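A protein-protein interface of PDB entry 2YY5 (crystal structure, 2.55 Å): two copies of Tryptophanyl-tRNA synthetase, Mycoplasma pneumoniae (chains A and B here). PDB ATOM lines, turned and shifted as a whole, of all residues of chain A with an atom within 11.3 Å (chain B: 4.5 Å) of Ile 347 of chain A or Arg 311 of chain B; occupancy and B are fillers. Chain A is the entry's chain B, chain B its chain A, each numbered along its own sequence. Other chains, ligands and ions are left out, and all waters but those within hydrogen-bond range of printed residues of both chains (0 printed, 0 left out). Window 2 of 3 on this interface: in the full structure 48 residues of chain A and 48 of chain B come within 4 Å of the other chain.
Of the 11 printed residues of chain A, 5 touch a printed residue of chain B.
Printed residues of chain A that touch a printed residue of chain B: Ser 344, Gln 345, Asn 346, Ile 347 and Lys 348.
Hydrophobic or aromatic side chains of chain A within 4 Å of the printed part of chain B: Ile 347.
Printed residues of chain B that touch a printed residue of chain A: Lys 58, Phe 62, Arg 311, Phe 315 and Leu 318.
Hydrophobic or aromatic side chains of chain B within 4 Å of the printed part of chain A: Phe 62, Phe 315 and Leu 318.
Along chain B the printed residues that touch a printed residue of chain A span positions 58 to 318.
Among the printed residues, 9 pairs touch across the chains.
Among the printed residues, no Asp or Glu carboxylate lies within 4 Å of a Lys or Arg side-chain nitrogen of the other chain.
The backbone carbonyl oxygen (O) of Leu 342 of chain A lies within hydrogen-bond range of the side-chain amide nitrogen (ND2) of Asn 346 of chain A, 2.4 Å away.
The backbone carbonyl oxygen of Gly 343 of chain A lies within hydrogen-bond range of the side-chain amide nitrogen of Asn 346 of chain A (3.3 Å).
Arg 311 of chain B touches just one residue of chain A: Ile 347.
No residue of chain A comes within 4 Å of Ser 310 of chain B.
Glu 312 of chain B touches none of the printed residues of chain A.
Gln 313 of chain B touches none of the printed residues of chain A.
No residue of chain A comes within 4 Å of Val 314 of chain B.
Of chain A, only Ser 344 (3.4 Å), Gln 345 (3.9 Å), Ile 347 (3.7 Å) and Lys 348 (3.7 Å) come within 4 Å of Phe 315 of chain B.
Printed residues of chain B within 4 Å of Gln 345 of chain A: Phe 315.
Of the printed residues of chain A, Lys 58 of chain B touches Asn 346.
Printed residues of chain B within 4 Å of Ser 344 of chain A: Phe 315 and Leu 318.
The nearest printed residue of chain B that does not touch Ser 344 of chain A is Val 314 of chain B (6.6 Å).
O of Ser 344 of chain A touches CD2 of Phe 315 of chain B (3.4 Å).
Leu 318 of chain B touches Ser 344 of chain A (CD1 to CB, 3.8 Å).
CE2 of Phe 315 of chain B touches CA of Gln 345 of chain A, 3.9 Å away.
Asn 346 of chain A touches Lys 58 of chain B.
CG2 of Ile 347 of chain A touches CD2 of Phe 62 of chain B (3.9 Å).
Ile 347 of chain A touches Arg 311 of chain B (CG2 to NE, 2.9 Å).
Ile 347 of chain A touches Phe 315 of chain B (O to CD2, 3.7 Å).
CD1 of Leu 318 of chain B touches CD1 of Ile 347 of chain A (3.9 Å).
Lys 348 of chain A touches Phe 315 of chain B.
No position is printed for both chains.
Of the 9 pairs that touch across the chains among the printed residues, none has its exchanged pair printed and touching as well.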
ATOM      1  N   TYR A 337      11.473  10.264  25.065  1.00  0.00           N
ATOM      2  CA  TYR A 337      12.367  11.173  24.371  1.00  0.00           C
ATOM      3  C   TYR A 337      13.245  11.851  25.401  1.00  0.00           C
ATOM      4  O   TYR A 337      14.450  11.977  25.203  1.00  0.00           O
ATOM      5  CB  TYR A 337      11.577  12.214  23.567  1.00  0.00           C
ATOM      6  CG  TYR A 337      11.524  11.905  22.085  1.00  0.00           C
ATOM      7  CD1 TYR A 337      11.197  10.623  21.631  1.00  0.00           C
ATOM      8  CD2 TYR A 337      11.800  12.886  21.135  1.00  0.00           C
ATOM      9  CE1 TYR A 337      11.152  10.328  20.271  1.00  0.00           C
ATOM     10  CE2 TYR A 337      11.754  12.596  19.770  1.00  0.00           C
ATOM     11  CZ  TYR A 337      11.429  11.315  19.349  1.00  0.00           C
ATOM     12  OH  TYR A 337      11.376  11.018  18.010  1.00  0.00           O
ATOM     13  N   ASP A 338      12.649  12.278  26.510  1.00  0.00           N
ATOM     14  CA  ASP A 338      13.434  12.928  27.552  1.00  0.00           C
ATOM     15  C   ASP A 338      14.522  12.001  28.048  1.00  0.00           C
ATOM     16  O   ASP A 338      15.690  12.381  28.090  1.00  0.00           O
ATOM     17  CB  ASP A 338      12.559  13.338  28.728  1.00  0.00           C
ATOM     18  CG  ASP A 338      12.005  14.729  28.573  1.00  0.00           C
ATOM     19  OD1 ASP A 338      10.910  14.872  27.991  1.00  0.00           O
ATOM     20  OD2 ASP A 338      12.679  15.682  29.024  1.00  0.00           O
ATOM     21  N   PHE A 340      15.793   9.314  26.641  1.00  0.00           N
ATOM     22  CA  PHE A 340      16.740   8.944  25.596  1.00  0.00           C
ATOM     23  C   PHE A 340      17.639  10.101  25.154  1.00  0.00           C
ATOM     24  O   PHE A 340      18.759   9.887  24.676  1.00  0.00           O
ATOM     25  CB  PHE A 340      15.984   8.387  24.384  1.00  0.00           C
ATOM     26  CG  PHE A 340      15.632   6.933  24.508  1.00  0.00           C
ATOM     27  CD1 PHE A 340      14.769   6.494  25.509  1.00  0.00           C
ATOM     28  CD2 PHE A 340      16.182   5.996  23.637  1.00  0.00           C
ATOM     29  CE1 PHE A 340      14.463   5.151  25.643  1.00  0.00           C
ATOM     30  CE2 PHE A 340      15.884   4.651  23.762  1.00  0.00           C
ATOM     31  CZ  PHE A 340      15.022   4.225  24.770  1.00  0.00           C
ATOM     32  N   GLY A 341      17.143  11.324  25.311  1.00  0.00           N
ATOM     33  CA  GLY A 341      17.913  12.491  24.910  1.00  0.00           C
ATOM     34  C   GLY A 341      17.644  12.890  23.471  1.00  0.00           C
ATOM     35  O   GLY A 341      18.434  13.620  22.870  1.00  0.00           O
ATOM     36  N   LEU A 342      16.529  12.406  22.924  1.00  0.00           N
ATOM     37  CA  LEU A 342      16.115  12.681  21.545  1.00  0.00           C
ATOM     38  C   LEU A 342      15.275  13.955  21.422  1.00  0.00           C
ATOM     39  O   LEU A 342      14.817  14.491  22.422  1.00  0.00           O
ATOM     40  CB  LEU A 342      15.319  11.488  20.993  1.00  0.00           C
ATOM     41  CG  LEU A 342      16.032  10.341  20.241  1.00  0.00           C
ATOM     42  CD1 LEU A 342      17.537  10.504  20.282  1.00  0.00           C
ATOM     43  CD2 LEU A 342      15.620   9.004  20.838  1.00  0.00           C
ATOM     44  N   GLY A 343      15.082  14.436  20.195  1.00  0.00           N
ATOM     45  CA  GLY A 343      14.286  15.634  19.984  1.00  0.00           C
ATOM     46  C   GLY A 343      15.038  16.926  20.240  1.00  0.00           C
ATOM     47  O   GLY A 343      16.040  16.931  20.946  1.00  0.00           O
ATOM     48  N   SER A 344      14.545  18.027  19.688  1.00  0.00           N
ATOM     49  CA  SER A 344      15.209  19.314  19.848  1.00  0.00           C
ATOM     50  C   SER A 344      14.676  20.156  20.995  1.00  0.00           C
ATOM     51  O   SER A 344      15.314  21.126  21.391  1.00  0.00           O
ATOM     52  CB  SER A 344      15.117  20.113  18.547  1.00  0.00           C
ATOM     53  OG  SER A 344      13.768  20.391  18.230  1.00  0.00           O
ATOM     54  N   GLN A 345      13.511  19.825  21.541  1.00  0.00           N
ATOM     55  CA  GLN A 345      13.010  20.626  22.650  1.00  0.00           C
ATOM     56  C   GLN A 345      13.702  20.197  23.938  1.00  0.00           C
ATOM     57  O   GLN A 345      13.214  20.461  25.037  1.00  0.00           O
ATOM     58  CB  GLN A 345      11.478  20.528  22.764  1.00  0.00           C
ATOM     59  CG  GLN A 345      10.866  19.165  23.088  1.00  0.00           C
ATOM     60  CD  GLN A 345       9.333  19.209  23.039  1.00  0.00           C
ATOM     61  OE1 GLN A 345       8.735  19.313  21.963  1.00  0.00           O
ATOM     62  NE2 GLN A 345       8.697  19.151  24.208  1.00  0.00           N
ATOM     63  N   ASN A 346      14.851  19.539  23.752  1.00  0.00           N
ATOM     64  CA  ASN A 346      15.721  19.033  24.799  1.00  0.00           C
ATOM     65  C   ASN A 346      16.847  20.030  24.999  1.00  0.00           C
ATOM     66  O   ASN A 346      17.660  19.851  25.947  1.00  0.00           O
ATOM     67  CB  ASN A 346      16.319  17.650  24.443  1.00  0.00           C
ATOM     68  CG  ASN A 346      15.305  16.504  24.585  1.00  0.00           C
ATOM     69  OD1 ASN A 346      15.432  15.647  25.467  1.00  0.00           O
ATOM     70  ND2 ASN A 346      14.312  16.482  23.707  1.00  0.00           N
ATOM     71  N   ILE A 347      16.972  21.032  24.118  1.00  0.00           N
ATOM     72  CA  ILE A 347      17.994  22.094  24.262  1.00  0.00           C
ATOM     73  C   ILE A 347      17.372  23.456  24.454  1.00  0.00           C
ATOM     74  O   ILE A 347      17.157  24.189  23.486  1.00  0.00           O
ATOM     75  CB  ILE A 347      18.801  22.367  22.975  1.00  0.00           C
ATOM     76  CG1 ILE A 347      18.650  21.128  22.074  1.00  0.00           C
ATOM     77  CG2 ILE A 347      20.238  22.580  23.363  1.00  0.00           C
ATOM     78  CD1 ILE A 347      18.189  21.386  20.727  1.00  0.00           C
ATOM     79  N   LYS A 348      17.118  23.836  25.682  1.00  0.00           N
ATOM     80  CA  LYS A 348      16.511  25.091  26.091  1.00  0.00           C
ATOM     81  C   LYS A 348      15.468  25.740  25.132  1.00  0.00           C
ATOM     82  O   LYS A 348      14.252  25.715  25.488  1.00  0.00           O
ATOM     83  CB  LYS A 348      17.559  26.160  26.454  1.00  0.00           C
ATOM     84  CG  LYS A 348      17.332  26.695  27.881  1.00  0.00           C
ATOM     85  CD  LYS A 348      18.077  27.994  28.180  1.00  0.00           C
ATOM     86  CE  LYS A 348      18.351  28.126  29.703  1.00  0.00           C
ATOM     87  NZ  LYS A 348      19.140  29.388  29.944  1.00  0.00           N
ATOM     88  OXT LYS A 348      15.862  26.255  24.041  1.00  0.00           O
ATOM     89  N   LYS B  58      22.445  14.732  23.439  1.00  0.00           N
ATOM     90  CA  LYS B  58      21.834  16.051  23.285  1.00  0.00           C
ATOM     91  C   LYS B  58      22.921  17.104  23.111  1.00  0.00           C
ATOM     92  O   LYS B  58      22.736  18.095  22.402  1.00  0.00           O
ATOM     93  CB  LYS B  58      20.931  16.380  24.493  1.00  0.00           C
ATOM     94  CG  LYS B  58      21.596  17.095  25.676  1.00  0.00           C
ATOM     95  CD  LYS B  58      21.937  18.566  25.353  1.00  0.00           C
ATOM     96  CE  LYS B  58      22.467  19.329  26.566  1.00  0.00           C
ATOM     97  NZ  LYS B  58      21.368  19.862  27.422  1.00  0.00           N
ATOM     98  N   PHE B  62      23.568  19.138  19.608  1.00  0.00           N
ATOM     99  CA  PHE B  62      23.683  20.585  19.743  1.00  0.00           C
ATOM    100  C   PHE B  62      24.983  21.102  19.126  1.00  0.00           C
ATOM    101  O   PHE B  62      24.971  22.077  18.385  1.00  0.00           O
ATOM    102  CB  PHE B  62      23.589  20.972  21.231  1.00  0.00           C
ATOM    103  CG  PHE B  62      24.097  22.357  21.544  1.00  0.00           C
ATOM    104  CD1 PHE B  62      25.307  22.532  22.216  1.00  0.00           C
ATOM    105  CD2 PHE B  62      23.356  23.486  21.193  1.00  0.00           C
ATOM    106  CE1 PHE B  62      25.775  23.811  22.543  1.00  0.00           C
ATOM    107  CE2 PHE B  62      23.810  24.772  21.511  1.00  0.00           C
ATOM    108  CZ  PHE B  62      25.022  24.935  22.189  1.00  0.00           C
ATOM    109  N   ILE B 309      27.513  31.240  17.860  1.00  0.00           N
ATOM    110  CA  ILE B 309      26.223  30.559  17.768  1.00  0.00           C
ATOM    111  C   ILE B 309      25.699  30.237  19.171  1.00  0.00           C
ATOM    112  O   ILE B 309      26.284  29.424  19.888  1.00  0.00           O
ATOM    113  CB  ILE B 309      26.337  29.230  16.980  1.00  0.00           C
ATOM    114  CG1 ILE B 309      27.166  29.430  15.705  1.00  0.00           C
ATOM    115  CG2 ILE B 309      24.943  28.717  16.646  1.00  0.00           C
ATOM    116  CD1 ILE B 309      26.584  30.433  14.739  1.00  0.00           C
ATOM    117  N   SER B 310      24.595  30.874  19.551  1.00  0.00           N
ATOM    118  CA  SER B 310      24.005  30.658  20.867  1.00  0.00           C
ATOM    119  C   SER B 310      23.113  29.431  20.916  1.00  0.00           C
ATOM    120  O   SER B 310      22.669  28.926  19.880  1.00  0.00           O
ATOM    121  CB  SER B 310      23.189  31.884  21.295  1.00  0.00           C
ATOM    122  OG  SER B 310      22.120  32.159  20.401  1.00  0.00           O
ATOM    123  N   ARG B 311      22.845  28.966  22.134  1.00  0.00           N
ATOM    124  CA  ARG B 311      21.996  27.801  22.357  1.00  0.00           C
ATOM    125  C   ARG B 311      20.630  28.092  21.763  1.00  0.00           C
ATOM    126  O   ARG B 311      19.919  27.193  21.325  1.00  0.00           O
ATOM    127  CB  ARG B 311      21.864  27.522  23.857  1.00  0.00           C
ATOM    128  CG  ARG B 311      21.370  26.117  24.193  1.00  0.00           C
ATOM    129  CD  ARG B 311      22.388  25.355  25.057  1.00  0.00           C
ATOM    130  NE  ARG B 311      22.237  23.905  24.922  1.00  0.00           N
ATOM    131  CZ  ARG B 311      23.109  23.003  25.365  1.00  0.00           C
ATOM    132  NH1 ARG B 311      24.216  23.386  25.987  1.00  0.00           N
ATOM    133  NH2 ARG B 311      22.886  21.711  25.158  1.00  0.00           N
ATOM    134  N   GLU B 312      20.277  29.368  21.740  1.00  0.00           N
ATOM    135  CA  GLU B 312      19.002  29.801  21.203  1.00  0.00           C
ATOM    136  C   GLU B 312      18.974  29.729  19.673  1.00  0.00           C
ATOM    137  O   GLU B 312      18.006  29.238  19.092  1.00  0.00           O
ATOM    138  CB  GLU B 312      18.714  31.230  21.666  1.00  0.00           C
ATOM    139  CG  GLU B 312      17.351  31.760  21.251  1.00  0.00           C
ATOM    140  CD  GLU B 312      16.442  32.023  22.433  1.00  0.00           C
ATOM    141  OE1 GLU B 312      16.740  32.945  23.225  1.00  0.00           O
ATOM    142  OE2 GLU B 312      15.432  31.303  22.572  1.00  0.00           O
ATOM    143  N   GLN B 313      20.028  30.216  19.020  1.00  0.00           N
ATOM    144  CA  GLN B 313      20.084  30.188  17.560  1.00  0.00           C
ATOM    145  C   GLN B 313      19.931  28.759  17.026  1.00  0.00           C
ATOM    146  O   GLN B 313      19.306  28.541  15.984  1.00  0.00           O
ATOM    147  CB  GLN B 313      21.409  30.760  17.054  1.00  0.00           C
ATOM    148  CG  GLN B 313      21.782  32.099  17.626  1.00  0.00           C
ATOM    149  CD  GLN B 313      23.117  32.585  17.103  1.00  0.00           C
ATOM    150  OE1 GLN B 313      23.832  33.328  17.782  1.00  0.00           O
ATOM    151  NE2 GLN B 313      23.457  32.177  15.883  1.00  0.00           N
ATOM    152  N   VAL B 314      20.521  27.798  17.738  1.00  0.00           N
ATOM    153  CA  VAL B 314      20.459  26.397  17.346  1.00  0.00           C
ATOM    154  C   VAL B 314      19.009  25.909  17.431  1.00  0.00           C
ATOM    155  O   VAL B 314      18.441  25.433  16.445  1.00  0.00           O
ATOM    156  CB  VAL B 314      21.367  25.503  18.270  1.00  0.00           C
ATOM    157  CG1 VAL B 314      21.152  24.027  17.973  1.00  0.00           C
ATOM    158  CG2 VAL B 314      22.832  25.848  18.070  1.00  0.00           C
ATOM    159  N   PHE B 315      18.415  26.047  18.612  1.00  0.00           N
ATOM    160  CA  PHE B 315      17.047  25.602  18.832  1.00  0.00           C
ATOM    161  C   PHE B 315      16.090  26.159  17.798  1.00  0.00           C
ATOM    162  O   PHE B 315      15.289  25.422  17.230  1.00  0.00           O
ATOM    163  CB  PHE B 315      16.567  25.998  20.234  1.00  0.00           C
ATOM    164  CG  PHE B 315      15.111  25.702  20.475  1.00  0.00           C
ATOM    165  CD1 PHE B 315      14.162  26.723  20.425  1.00  0.00           C
ATOM    166  CD2 PHE B 315      14.684  24.396  20.728  1.00  0.00           C
ATOM    167  CE1 PHE B 315      12.814  26.449  20.627  1.00  0.00           C
ATOM    168  CE2 PHE B 315      13.330  24.109  20.931  1.00  0.00           C
ATOM    169  CZ  PHE B 315      12.395  25.142  20.879  1.00  0.00           C
ATOM    170  N   LEU B 318      16.605  24.600  14.427  1.00  0.00           N
ATOM    171  CA  LEU B 318      16.025  23.270  14.395  1.00  0.00           C
ATOM    172  C   LEU B 318      14.501  23.321  14.340  1.00  0.00           C
ATOM    173  O   LEU B 318      13.860  22.468  13.711  1.00  0.00           O
ATOM    174  CB  LEU B 318      16.483  22.473  15.620  1.00  0.00           C
ATOM    175  CG  LEU B 318      17.955  22.078  15.605  1.00  0.00           C
ATOM    176  CD1 LEU B 318      18.286  21.294  16.847  1.00  0.00           C
ATOM    177  CD2 LEU B 318      18.236  21.244  14.360  1.00  0.00           C
